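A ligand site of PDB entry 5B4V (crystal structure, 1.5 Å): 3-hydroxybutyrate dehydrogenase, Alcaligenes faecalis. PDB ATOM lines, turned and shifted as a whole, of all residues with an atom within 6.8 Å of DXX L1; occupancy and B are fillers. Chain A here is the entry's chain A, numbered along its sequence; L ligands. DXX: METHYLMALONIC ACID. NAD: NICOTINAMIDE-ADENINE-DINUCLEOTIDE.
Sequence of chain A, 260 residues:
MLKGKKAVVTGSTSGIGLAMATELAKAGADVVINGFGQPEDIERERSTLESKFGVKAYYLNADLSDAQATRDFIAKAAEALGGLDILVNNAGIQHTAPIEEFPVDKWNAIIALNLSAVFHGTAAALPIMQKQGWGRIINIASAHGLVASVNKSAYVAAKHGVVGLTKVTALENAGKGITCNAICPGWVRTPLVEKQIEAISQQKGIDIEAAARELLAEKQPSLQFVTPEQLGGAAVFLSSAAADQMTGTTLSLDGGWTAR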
ATOM      1  N   GLN A  94     -28.410 -10.638 -16.878  1.00  0.00           N
ATOM      2  CA  GLN A  94     -29.633  -9.860 -16.671  1.00  0.00           C
ATOM      3  C   GLN A  94     -30.836 -10.816 -16.546  1.00  0.00           C
ATOM      4  O   GLN A  94     -30.831 -11.894 -17.128  1.00  0.00           O
ATOM      5  CB  GLN A  94     -29.850  -8.921 -17.867  1.00  0.00           C
ATOM      6  CG  GLN A  94     -31.090  -8.042 -17.796  1.00  0.00           C
ATOM      7  CD  GLN A  94     -31.108  -7.118 -16.592  1.00  0.00           C
ATOM      8  OE1 GLN A  94     -31.306  -7.564 -15.466  1.00  0.00           O
ATOM      9  NE2 GLN A  94     -30.797  -5.847 -16.824  1.00  0.00           N
ATOM     10  N   THR A  96     -35.307 -10.078 -15.961  1.00  0.00           N
ATOM     11  CA  THR A  96     -36.333  -9.076 -15.699  1.00  0.00           C
ATOM     12  C   THR A  96     -37.618  -9.695 -15.126  1.00  0.00           C
ATOM     13  O   THR A  96     -38.121 -10.717 -15.613  1.00  0.00           O
ATOM     14  CB  THR A  96     -36.699  -8.282 -16.971  1.00  0.00           C
ATOM     15  OG1 THR A  96     -37.302  -9.163 -17.898  1.00  0.00           O
ATOM     16  CG2 THR A  96     -35.487  -7.652 -17.616  1.00  0.00           C
ATOM     17  N   ALA A 141     -20.049  -1.270 -15.198  1.00  0.00           N
ATOM     18  CA  ALA A 141     -21.297  -1.138 -14.492  1.00  0.00           C
ATOM     19  C   ALA A 141     -22.419  -0.964 -15.493  1.00  0.00           C
ATOM     20  O   ALA A 141     -22.598  -1.850 -16.330  1.00  0.00           O
ATOM     21  CB  ALA A 141     -21.227  -0.017 -13.470  1.00  0.00           C
ATOM     22  N   SER A 142     -23.126   0.169 -15.467  1.00  0.00           N
ATOM     23  CA  SER A 142     -24.286   0.413 -16.339  1.00  0.00           C
ATOM     24  C   SER A 142     -24.827   1.801 -15.987  1.00  0.00           C
ATOM     25  O   SER A 142     -24.599   2.310 -14.879  1.00  0.00           O
ATOM     26  CB  SER A 142     -25.382  -0.623 -16.086  1.00  0.00           C
ATOM     27  OG  SER A 142     -26.557  -0.350 -16.832  1.00  0.00           O
ATOM     28  N   ALA A 143     -25.653   2.353 -16.859  1.00  0.00           N
ATOM     29  CA  ALA A 143     -26.565   3.413 -16.450  1.00  0.00           C
ATOM     30  C   ALA A 143     -27.360   3.005 -15.211  1.00  0.00           C
ATOM     31  O   ALA A 143     -27.659   3.831 -14.346  1.00  0.00           O
ATOM     32  CB  ALA A 143     -27.506   3.766 -17.591  1.00  0.00           C
ATOM     33  N   HIS A 144     -27.624   1.699 -15.096  1.00  0.00           N
ATOM     34  CA  HIS A 144     -28.350   1.132 -13.977  1.00  0.00           C
ATOM     35  C   HIS A 144     -27.509   0.958 -12.710  1.00  0.00           C
ATOM     36  O   HIS A 144     -28.021   0.508 -11.696  1.00  0.00           O
ATOM     37  CB  HIS A 144     -28.973  -0.191 -14.370  1.00  0.00           C
ATOM     38  CG  HIS A 144     -30.208  -0.052 -15.196  1.00  0.00           C
ATOM     39  ND1 HIS A 144     -30.321  -0.592 -16.453  1.00  0.00           N
ATOM     40  CD2 HIS A 144     -31.282   0.742 -15.028  1.00  0.00           C
ATOM     41  CE1 HIS A 144     -31.508  -0.284 -16.950  1.00  0.00           C
ATOM     42  NE2 HIS A 144     -32.098   0.548 -16.108  1.00  0.00           N
ATOM     43  N   GLY A 145     -26.291   1.478 -12.724  1.00  0.00           N
ATOM     44  CA  GLY A 145     -25.541   1.723 -11.500  1.00  0.00           C
ATOM     45  C   GLY A 145     -25.764   3.112 -10.921  1.00  0.00           C
ATOM     46  O   GLY A 145     -25.261   3.419  -9.837  1.00  0.00           O
ATOM     47  N   SER A 149     -34.598   1.197 -13.428  1.00  0.00           N
ATOM     48  CA  SER A 149     -35.781   0.924 -14.222  1.00  0.00           C
ATOM     49  C   SER A 149     -36.601  -0.142 -13.518  1.00  0.00           C
ATOM     50  O   SER A 149     -36.082  -0.890 -12.694  1.00  0.00           O
ATOM     51  CB  SER A 149     -35.398   0.383 -15.597  1.00  0.00           C
ATOM     52  OG  SER A 149     -34.710   1.346 -16.375  1.00  0.00           O
ATOM     53  N   LYS A 152     -35.970  -4.701 -12.718  1.00  0.00           N
ATOM     54  CA  LYS A 152     -34.552  -4.997 -12.735  1.00  0.00           C
ATOM     55  C   LYS A 152     -33.914  -4.831 -11.345  1.00  0.00           C
ATOM     56  O   LYS A 152     -32.769  -4.406 -11.223  1.00  0.00           O
ATOM     57  CB  LYS A 152     -33.851  -4.117 -13.782  1.00  0.00           C
ATOM     58  CG  LYS A 152     -34.254  -4.508 -15.199  1.00  0.00           C
ATOM     59  CD  LYS A 152     -33.654  -3.618 -16.276  1.00  0.00           C
ATOM     60  CE  LYS A 152     -34.021  -4.181 -17.644  1.00  0.00           C
ATOM     61  NZ  LYS A 152     -33.583  -3.296 -18.766  1.00  0.00           N
ATOM     62  N   TYR A 155     -30.339  -6.504 -10.782  1.00  0.00           N
ATOM     63  CA  TYR A 155     -29.324  -5.942 -11.652  1.00  0.00           C
ATOM     64  C   TYR A 155     -28.983  -4.498 -11.226  1.00  0.00           C
ATOM     65  O   TYR A 155     -27.808  -4.132 -11.142  1.00  0.00           O
ATOM     66  CB  TYR A 155     -29.837  -5.954 -13.102  1.00  0.00           C
ATOM     67  CG  TYR A 155     -28.825  -5.501 -14.131  1.00  0.00           C
ATOM     68  CD1 TYR A 155     -28.772  -4.177 -14.542  1.00  0.00           C
ATOM     69  CD2 TYR A 155     -27.933  -6.403 -14.700  1.00  0.00           C
ATOM     70  CE1 TYR A 155     -27.867  -3.774 -15.506  1.00  0.00           C
ATOM     71  CE2 TYR A 155     -27.099  -6.030 -15.736  1.00  0.00           C
ATOM     72  CZ  TYR A 155     -27.045  -4.704 -16.096  1.00  0.00           C
ATOM     73  OH  TYR A 155     -26.170  -4.299 -17.090  1.00  0.00           O
ATOM     74  N   LYS A 159     -25.378  -3.324  -9.854  1.00  0.00           N
ATOM     75  CA  LYS A 159     -24.618  -2.313 -10.564  1.00  0.00           C
ATOM     76  C   LYS A 159     -24.377  -1.063  -9.721  1.00  0.00           C
ATOM     77  O   LYS A 159     -23.303  -0.481  -9.796  1.00  0.00           O
ATOM     78  CB  LYS A 159     -25.286  -1.954 -11.899  1.00  0.00           C
ATOM     79  CG  LYS A 159     -25.325  -3.101 -12.906  1.00  0.00           C
ATOM     80  CD  LYS A 159     -23.928  -3.549 -13.308  1.00  0.00           C
ATOM     81  CE  LYS A 159     -23.944  -4.399 -14.589  1.00  0.00           C
ATOM     82  NZ  LYS A 159     -22.597  -4.850 -14.999  1.00  0.00           N
ATOM     83  N   PRO A 185     -22.394   1.963 -19.417  1.00  0.00           N
ATOM     84  CA  PRO A 185     -23.075   2.053 -20.710  1.00  0.00           C
ATOM     85  C   PRO A 185     -24.584   2.163 -20.597  1.00  0.00           C
ATOM     86  O   PRO A 185     -25.198   1.617 -19.671  1.00  0.00           O
ATOM     87  CB  PRO A 185     -22.688   0.743 -21.415  1.00  0.00           C
ATOM     88  CG  PRO A 185     -21.593   0.145 -20.602  1.00  0.00           C
ATOM     89  CD  PRO A 185     -21.784   0.646 -19.203  1.00  0.00           C
ATOM     90  N   GLY A 186     -25.177   2.856 -21.560  1.00  0.00           N
ATOM     91  CA  GLY A 186     -26.577   2.664 -21.924  1.00  0.00           C
ATOM     92  C   GLY A 186     -26.759   1.424 -22.781  1.00  0.00           C
ATOM     93  O   GLY A 186     -25.954   0.496 -22.735  1.00  0.00           O
ATOM     94  N   TRP A 187     -27.819   1.409 -23.587  1.00  0.00           N
ATOM     95  CA  TRP A 187     -28.102   0.253 -24.420  1.00  0.00           C
ATOM     96  C   TRP A 187     -27.002   0.014 -25.436  1.00  0.00           C
ATOM     97  O   TRP A 187     -26.632   0.917 -26.201  1.00  0.00           O
ATOM     98  CB  TRP A 187     -29.415   0.432 -25.191  1.00  0.00           C
ATOM     99  CG  TRP A 187     -30.659   0.540 -24.366  1.00  0.00           C
ATOM    100  CD1 TRP A 187     -31.535   1.578 -24.373  1.00  0.00           C
ATOM    101  CD2 TRP A 187     -31.286  -0.491 -23.584  1.00  0.00           C
ATOM    102  NE1 TRP A 187     -32.673   1.261 -23.669  1.00  0.00           N
ATOM    103  CE2 TRP A 187     -32.502   0.020 -23.110  1.00  0.00           C
ATOM    104  CE3 TRP A 187     -30.963  -1.823 -23.306  1.00  0.00           C
ATOM    105  CZ2 TRP A 187     -33.397  -0.750 -22.360  1.00  0.00           C
ATOM    106  CZ3 TRP A 187     -31.869  -2.590 -22.587  1.00  0.00           C
ATOM    107  CH2 TRP A 187     -33.045  -2.031 -22.084  1.00  0.00           C
ATOM    108  N   VAL A 188     -26.583  -1.252 -25.505  1.00  0.00           N
ATOM    109  CA  VAL A 188     -25.594  -1.776 -26.451  1.00  0.00           C
ATOM    110  C   VAL A 188     -26.204  -3.054 -27.010  1.00  0.00           C
ATOM    111  O   VAL A 188     -26.717  -3.881 -26.248  1.00  0.00           O
ATOM    112  CB  VAL A 188     -24.288  -2.130 -25.722  1.00  0.00           C
ATOM    113  CG1 VAL A 188     -23.231  -2.608 -26.702  1.00  0.00           C
ATOM    114  CG2 VAL A 188     -23.767  -0.943 -24.924  1.00  0.00           C
ATOM    115  N   LEU A 192     -27.481  -9.824 -24.571  1.00  0.00           N
ATOM    116  CA  LEU A 192     -28.144  -9.484 -23.315  1.00  0.00           C
ATOM    117  C   LEU A 192     -29.356  -8.572 -23.550  1.00  0.00           C
ATOM    118  O   LEU A 192     -30.349  -8.619 -22.810  1.00  0.00           O
ATOM    119  CB  LEU A 192     -27.136  -8.796 -22.386  1.00  0.00           C
ATOM    120  CG  LEU A 192     -27.585  -8.376 -20.990  1.00  0.00           C
ATOM    121  CD1 LEU A 192     -26.389  -8.411 -20.064  1.00  0.00           C
ATOM    122  CD2 LEU A 192     -28.210  -6.981 -20.996  1.00  0.00           C
ATOM    123  N   VAL A 193     -29.244  -7.714 -24.563  1.00  0.00           N
ATOM    124  CA  VAL A 193     -30.262  -6.741 -24.921  1.00  0.00           C
ATOM    125  C   VAL A 193     -31.208  -7.295 -25.986  1.00  0.00           C
ATOM    126  O   VAL A 193     -32.388  -6.978 -26.002  1.00  0.00           O
ATOM    127  CB  VAL A 193     -29.580  -5.442 -25.397  1.00  0.00           C
ATOM    128  CG1 VAL A 193     -30.541  -4.543 -26.171  1.00  0.00           C
ATOM    129  CG2 VAL A 193     -29.004  -4.706 -24.199  1.00  0.00           C
ATOM    130  N   GLN A 196     -34.265  -8.737 -24.591  1.00  0.00           N
ATOM    131  CA  GLN A 196     -35.254  -7.766 -24.159  1.00  0.00           C
ATOM    132  C   GLN A 196     -35.993  -7.126 -25.332  1.00  0.00           C
ATOM    133  O   GLN A 196     -37.169  -6.783 -25.231  1.00  0.00           O
ATOM    134  CB  GLN A 196     -34.559  -6.678 -23.323  1.00  0.00           C
ATOM    135  CG  GLN A 196     -33.889  -7.207 -22.061  1.00  0.00           C
ATOM    136  CD  GLN A 196     -33.235  -6.113 -21.236  1.00  0.00           C
ATOM    137  OE1 GLN A 196     -33.911  -5.188 -20.782  1.00  0.00           O
ATOM    138  NE2 GLN A 196     -31.911  -6.138 -21.179  1.00  0.00           N
ATOM    139  N   GLN A 220     -32.973   6.350 -24.088  1.00  0.00           N
ATOM    140  CA  GLN A 220     -31.683   6.787 -24.650  1.00  0.00           C
ATOM    141  C   GLN A 220     -31.898   7.907 -25.684  1.00  0.00           C
ATOM    142  O   GLN A 220     -32.243   7.621 -26.829  1.00  0.00           O
ATOM    143  CB  GLN A 220     -31.016   5.560 -25.301  1.00  0.00           C
ATOM    144  CG  GLN A 220     -29.552   5.716 -25.680  1.00  0.00           C
ATOM    145  CD  GLN A 220     -28.758   4.471 -25.314  1.00  0.00           C
ATOM    146  OE1 GLN A 220     -28.894   3.942 -24.202  1.00  0.00           O
ATOM    147  NE2 GLN A 220     -27.979   3.951 -26.255  1.00  0.00           N
ATOM    148  N   TRP A 257     -28.888   9.084 -21.449  1.00  0.00           N
ATOM    149  CA  TRP A 257     -29.818   8.433 -20.489  1.00  0.00           C
ATOM    150  C   TRP A 257     -29.855   9.116 -19.126  1.00  0.00           C
ATOM    151  O   TRP A 257     -30.916   9.467 -18.609  1.00  0.00           O
ATOM    152  CB  TRP A 257     -29.387   6.973 -20.339  1.00  0.00           C
ATOM    153  CG  TRP A 257     -30.308   6.035 -19.600  1.00  0.00           C
ATOM    154  CD1 TRP A 257     -30.961   6.252 -18.429  1.00  0.00           C
ATOM    155  CD2 TRP A 257     -30.496   4.653 -19.911  1.00  0.00           C
ATOM    156  NE1 TRP A 257     -31.577   5.087 -18.006  1.00  0.00           N
ATOM    157  CE2 TRP A 257     -31.265   4.084 -18.883  1.00  0.00           C
ATOM    158  CE3 TRP A 257     -30.033   3.834 -20.948  1.00  0.00           C
ATOM    159  CZ2 TRP A 257     -31.684   2.757 -18.922  1.00  0.00           C
ATOM    160  CZ3 TRP A 257     -30.443   2.527 -20.992  1.00  0.00           C
ATOM    161  CH2 TRP A 257     -31.192   1.975 -19.937  1.00  0.00           C
HETATM  162  C1  DXX L   1     -30.416  -3.219 -19.416  1.00  0.00           C
HETATM  163  O1  DXX L   1     -30.578  -4.457 -19.463  1.00  0.00           O
HETATM  164  OXT DXX L   1     -31.161  -2.467 -18.766  1.00  0.00           O
HETATM  165  CA  DXX L   1     -29.181  -2.630 -20.022  1.00  0.00           C
HETATM  166  CB  DXX L   1     -29.381  -1.164 -20.406  1.00  0.00           C
HETATM  167  C   DXX L   1     -28.081  -2.767 -19.039  1.00  0.00           C
HETATM  168  O   DXX L   1     -28.034  -1.967 -18.065  1.00  0.00           O
HETATM  169  O2  DXX L   1     -27.427  -3.818 -19.103  1.00  0.00           O
HETATM  170  PA  NAD L   2     -23.178 -10.659 -23.238  1.00  0.00           P
HETATM  171  O1A NAD L   2     -24.218 -11.600 -22.762  1.00  0.00           O
HETATM  172  O2A NAD L   2     -22.937 -10.434 -24.704  1.00  0.00           O
HETATM  173  O5B NAD L   2     -21.783 -11.134 -22.648  1.00  0.00           O
HETATM  174  C5B NAD L   2     -21.682 -11.658 -21.328  1.00  0.00           C
HETATM  175  C4B NAD L   2     -20.301 -12.259 -21.191  1.00  0.00           C
HETATM  176  O4B NAD L   2     -20.150 -12.746 -19.850  1.00  0.00           O
HETATM  177  C3B NAD L   2     -20.163 -13.506 -22.077  1.00  0.00           C
HETATM  178  O3B NAD L   2     -18.783 -13.624 -22.472  1.00  0.00           O
HETATM  179  C2B NAD L   2     -20.582 -14.630 -21.147  1.00  0.00           C
HETATM  180  O2B NAD L   2     -20.105 -15.929 -21.549  1.00  0.00           O
HETATM  181  C1B NAD L   2     -19.916 -14.160 -19.869  1.00  0.00           C
HETATM  182  N9A NAD L   2     -20.447 -14.818 -18.684  1.00  0.00           N
HETATM  183  C8A NAD L   2     -21.742 -14.940 -18.317  1.00  0.00           C
HETATM  184  N7A NAD L   2     -21.843 -15.655 -17.173  1.00  0.00           N
HETATM  185  C5A NAD L   2     -20.580 -15.869 -16.721  1.00  0.00           C
HETATM  186  C6A NAD L   2     -19.961 -16.540 -15.579  1.00  0.00           C
HETATM  187  N6A NAD L   2     -20.723 -17.069 -14.601  1.00  0.00           N
HETATM  188  N1A NAD L   2     -18.617 -16.545 -15.527  1.00  0.00           N
HETATM  189  C2A NAD L   2     -17.835 -16.000 -16.478  1.00  0.00           C
HETATM  190  N3A NAD L   2     -18.340 -15.431 -17.591  1.00  0.00           N
HETATM  191  C4A NAD L   2     -19.679 -15.307 -17.711  1.00  0.00           C
HETATM  192  O3  NAD L   2     -23.524  -9.271 -22.470  1.00  0.00           O
HETATM  193  PN  NAD L   2     -22.934  -7.796 -22.614  1.00  0.00           P
HETATM  194  O1N NAD L   2     -24.110  -6.956 -22.988  1.00  0.00           O
HETATM  195  O2N NAD L   2     -21.705  -7.776 -23.458  1.00  0.00           O
HETATM  196  O5D NAD L   2     -22.546  -7.483 -21.087  1.00  0.00           O
HETATM  197  C5D NAD L   2     -21.214  -7.244 -20.639  1.00  0.00           C
HETATM  198  C4D NAD L   2     -21.312  -6.322 -19.432  1.00  0.00           C
HETATM  199  O4D NAD L   2     -21.899  -5.076 -19.867  1.00  0.00           O
HETATM  200  C3D NAD L   2     -22.219  -6.866 -18.323  1.00  0.00           C
HETATM  201  O3D NAD L   2     -21.618  -6.582 -17.042  1.00  0.00           O
HETATM  202  C2D NAD L   2     -23.495  -6.045 -18.453  1.00  0.00           C
HETATM  203  O2D NAD L   2     -24.162  -5.941 -17.193  1.00  0.00           O
HETATM  204  C1D NAD L   2     -22.914  -4.719 -18.932  1.00  0.00           C
HETATM  205  N1N NAD L   2     -23.860  -3.818 -19.563  1.00  0.00           N
HETATM  206  C2N NAD L   2     -24.465  -4.157 -20.729  1.00  0.00           C
HETATM  207  C3N NAD L   2     -25.292  -3.233 -21.369  1.00  0.00           C
HETATM  208  C7N NAD L   2     -25.974  -3.526 -22.677  1.00  0.00           C
HETATM  209  O7N NAD L   2     -26.790  -2.730 -23.113  1.00  0.00           O
HETATM  210  N7N NAD L   2     -25.623  -4.602 -23.383  1.00  0.00           N
HETATM  211  C4N NAD L   2     -25.541  -1.996 -20.775  1.00  0.00           C
HETATM  212  C5N NAD L   2     -24.913  -1.688 -19.572  1.00  0.00           C
HETATM  213  C6N NAD L   2     -24.020  -2.599 -19.019  1.00  0.00           C
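The side-chain amide nitrogen of Gln 196 sits at hydrogen-bond distance from an oxygen (O1) of DXX L1 (2.7 Å). O7N of NAD L2 lies within hydrogen-bond range of N of Val 188, at 2.8 Å. O of DXX L1 lies within hydrogen-bond range of OG of Ser 142, at 2.5 Å. OXT of DXX L1 lies close to ND1 of His 144. A nitrogen (N7N) of NAD L2 is in hydrogen-bond range of the backbone carbonyl oxygen of Val 188 (3.2 Å). O1 of DXX L1 lies within hydrogen-bond range of NE2 of Gln 94 (3.0 Å). O2D of NAD L2 lies within hydrogen-bond range of OH of Tyr 155. NZ of Lys 152 lies within salt-bridge range of OXT of DXX L1 (2.6 Å). The side-chain amino group of Lys 159 is in hydrogen-bond range of an oxygen (O3D) of NAD L2 (2.9 Å). OH of Tyr 155 is in hydrogen-bond range of O2 of DXX L1.
The side-chain amino group (NZ) of Lys 152 is in hydrogen-bond range of the side-chain amide oxygen (OE1) of Gln 196, at 2.8 Å. OG of Ser 142 sits at hydrogen-bond distance from N of His 144. The backbone carbonyl oxygen (O) of Leu 192 is in hydrogen-bond range of the side-chain amide nitrogen (NE2) of Gln 196 (3.4 Å). The backbone NH of Trp 187 sits at hydrogen-bond distance from the side-chain amide oxygen of Gln 220. A ring nitrogen (NE2) of His 144 lies within hydrogen-bond range of the side-chain hydroxyl (OG) of Ser 149.
Merely in contact with DXX L1: Trp 187, Leu 192 and Trp 257. Hydrophobic or aromatic side chains that line DXX L1: His 144, Tyr 155, Trp 187, Leu 192 and Trp 257. Nine residues have an atom within 4 Å of DXX L1: Gln 94, Ser 142, His 144, Lys 152, Tyr 155, Trp 187, Leu 192, Gln 196 and Trp 257. The nearest printed residue that does not touch DXX L1 is Gly 186 (4.4 Å).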
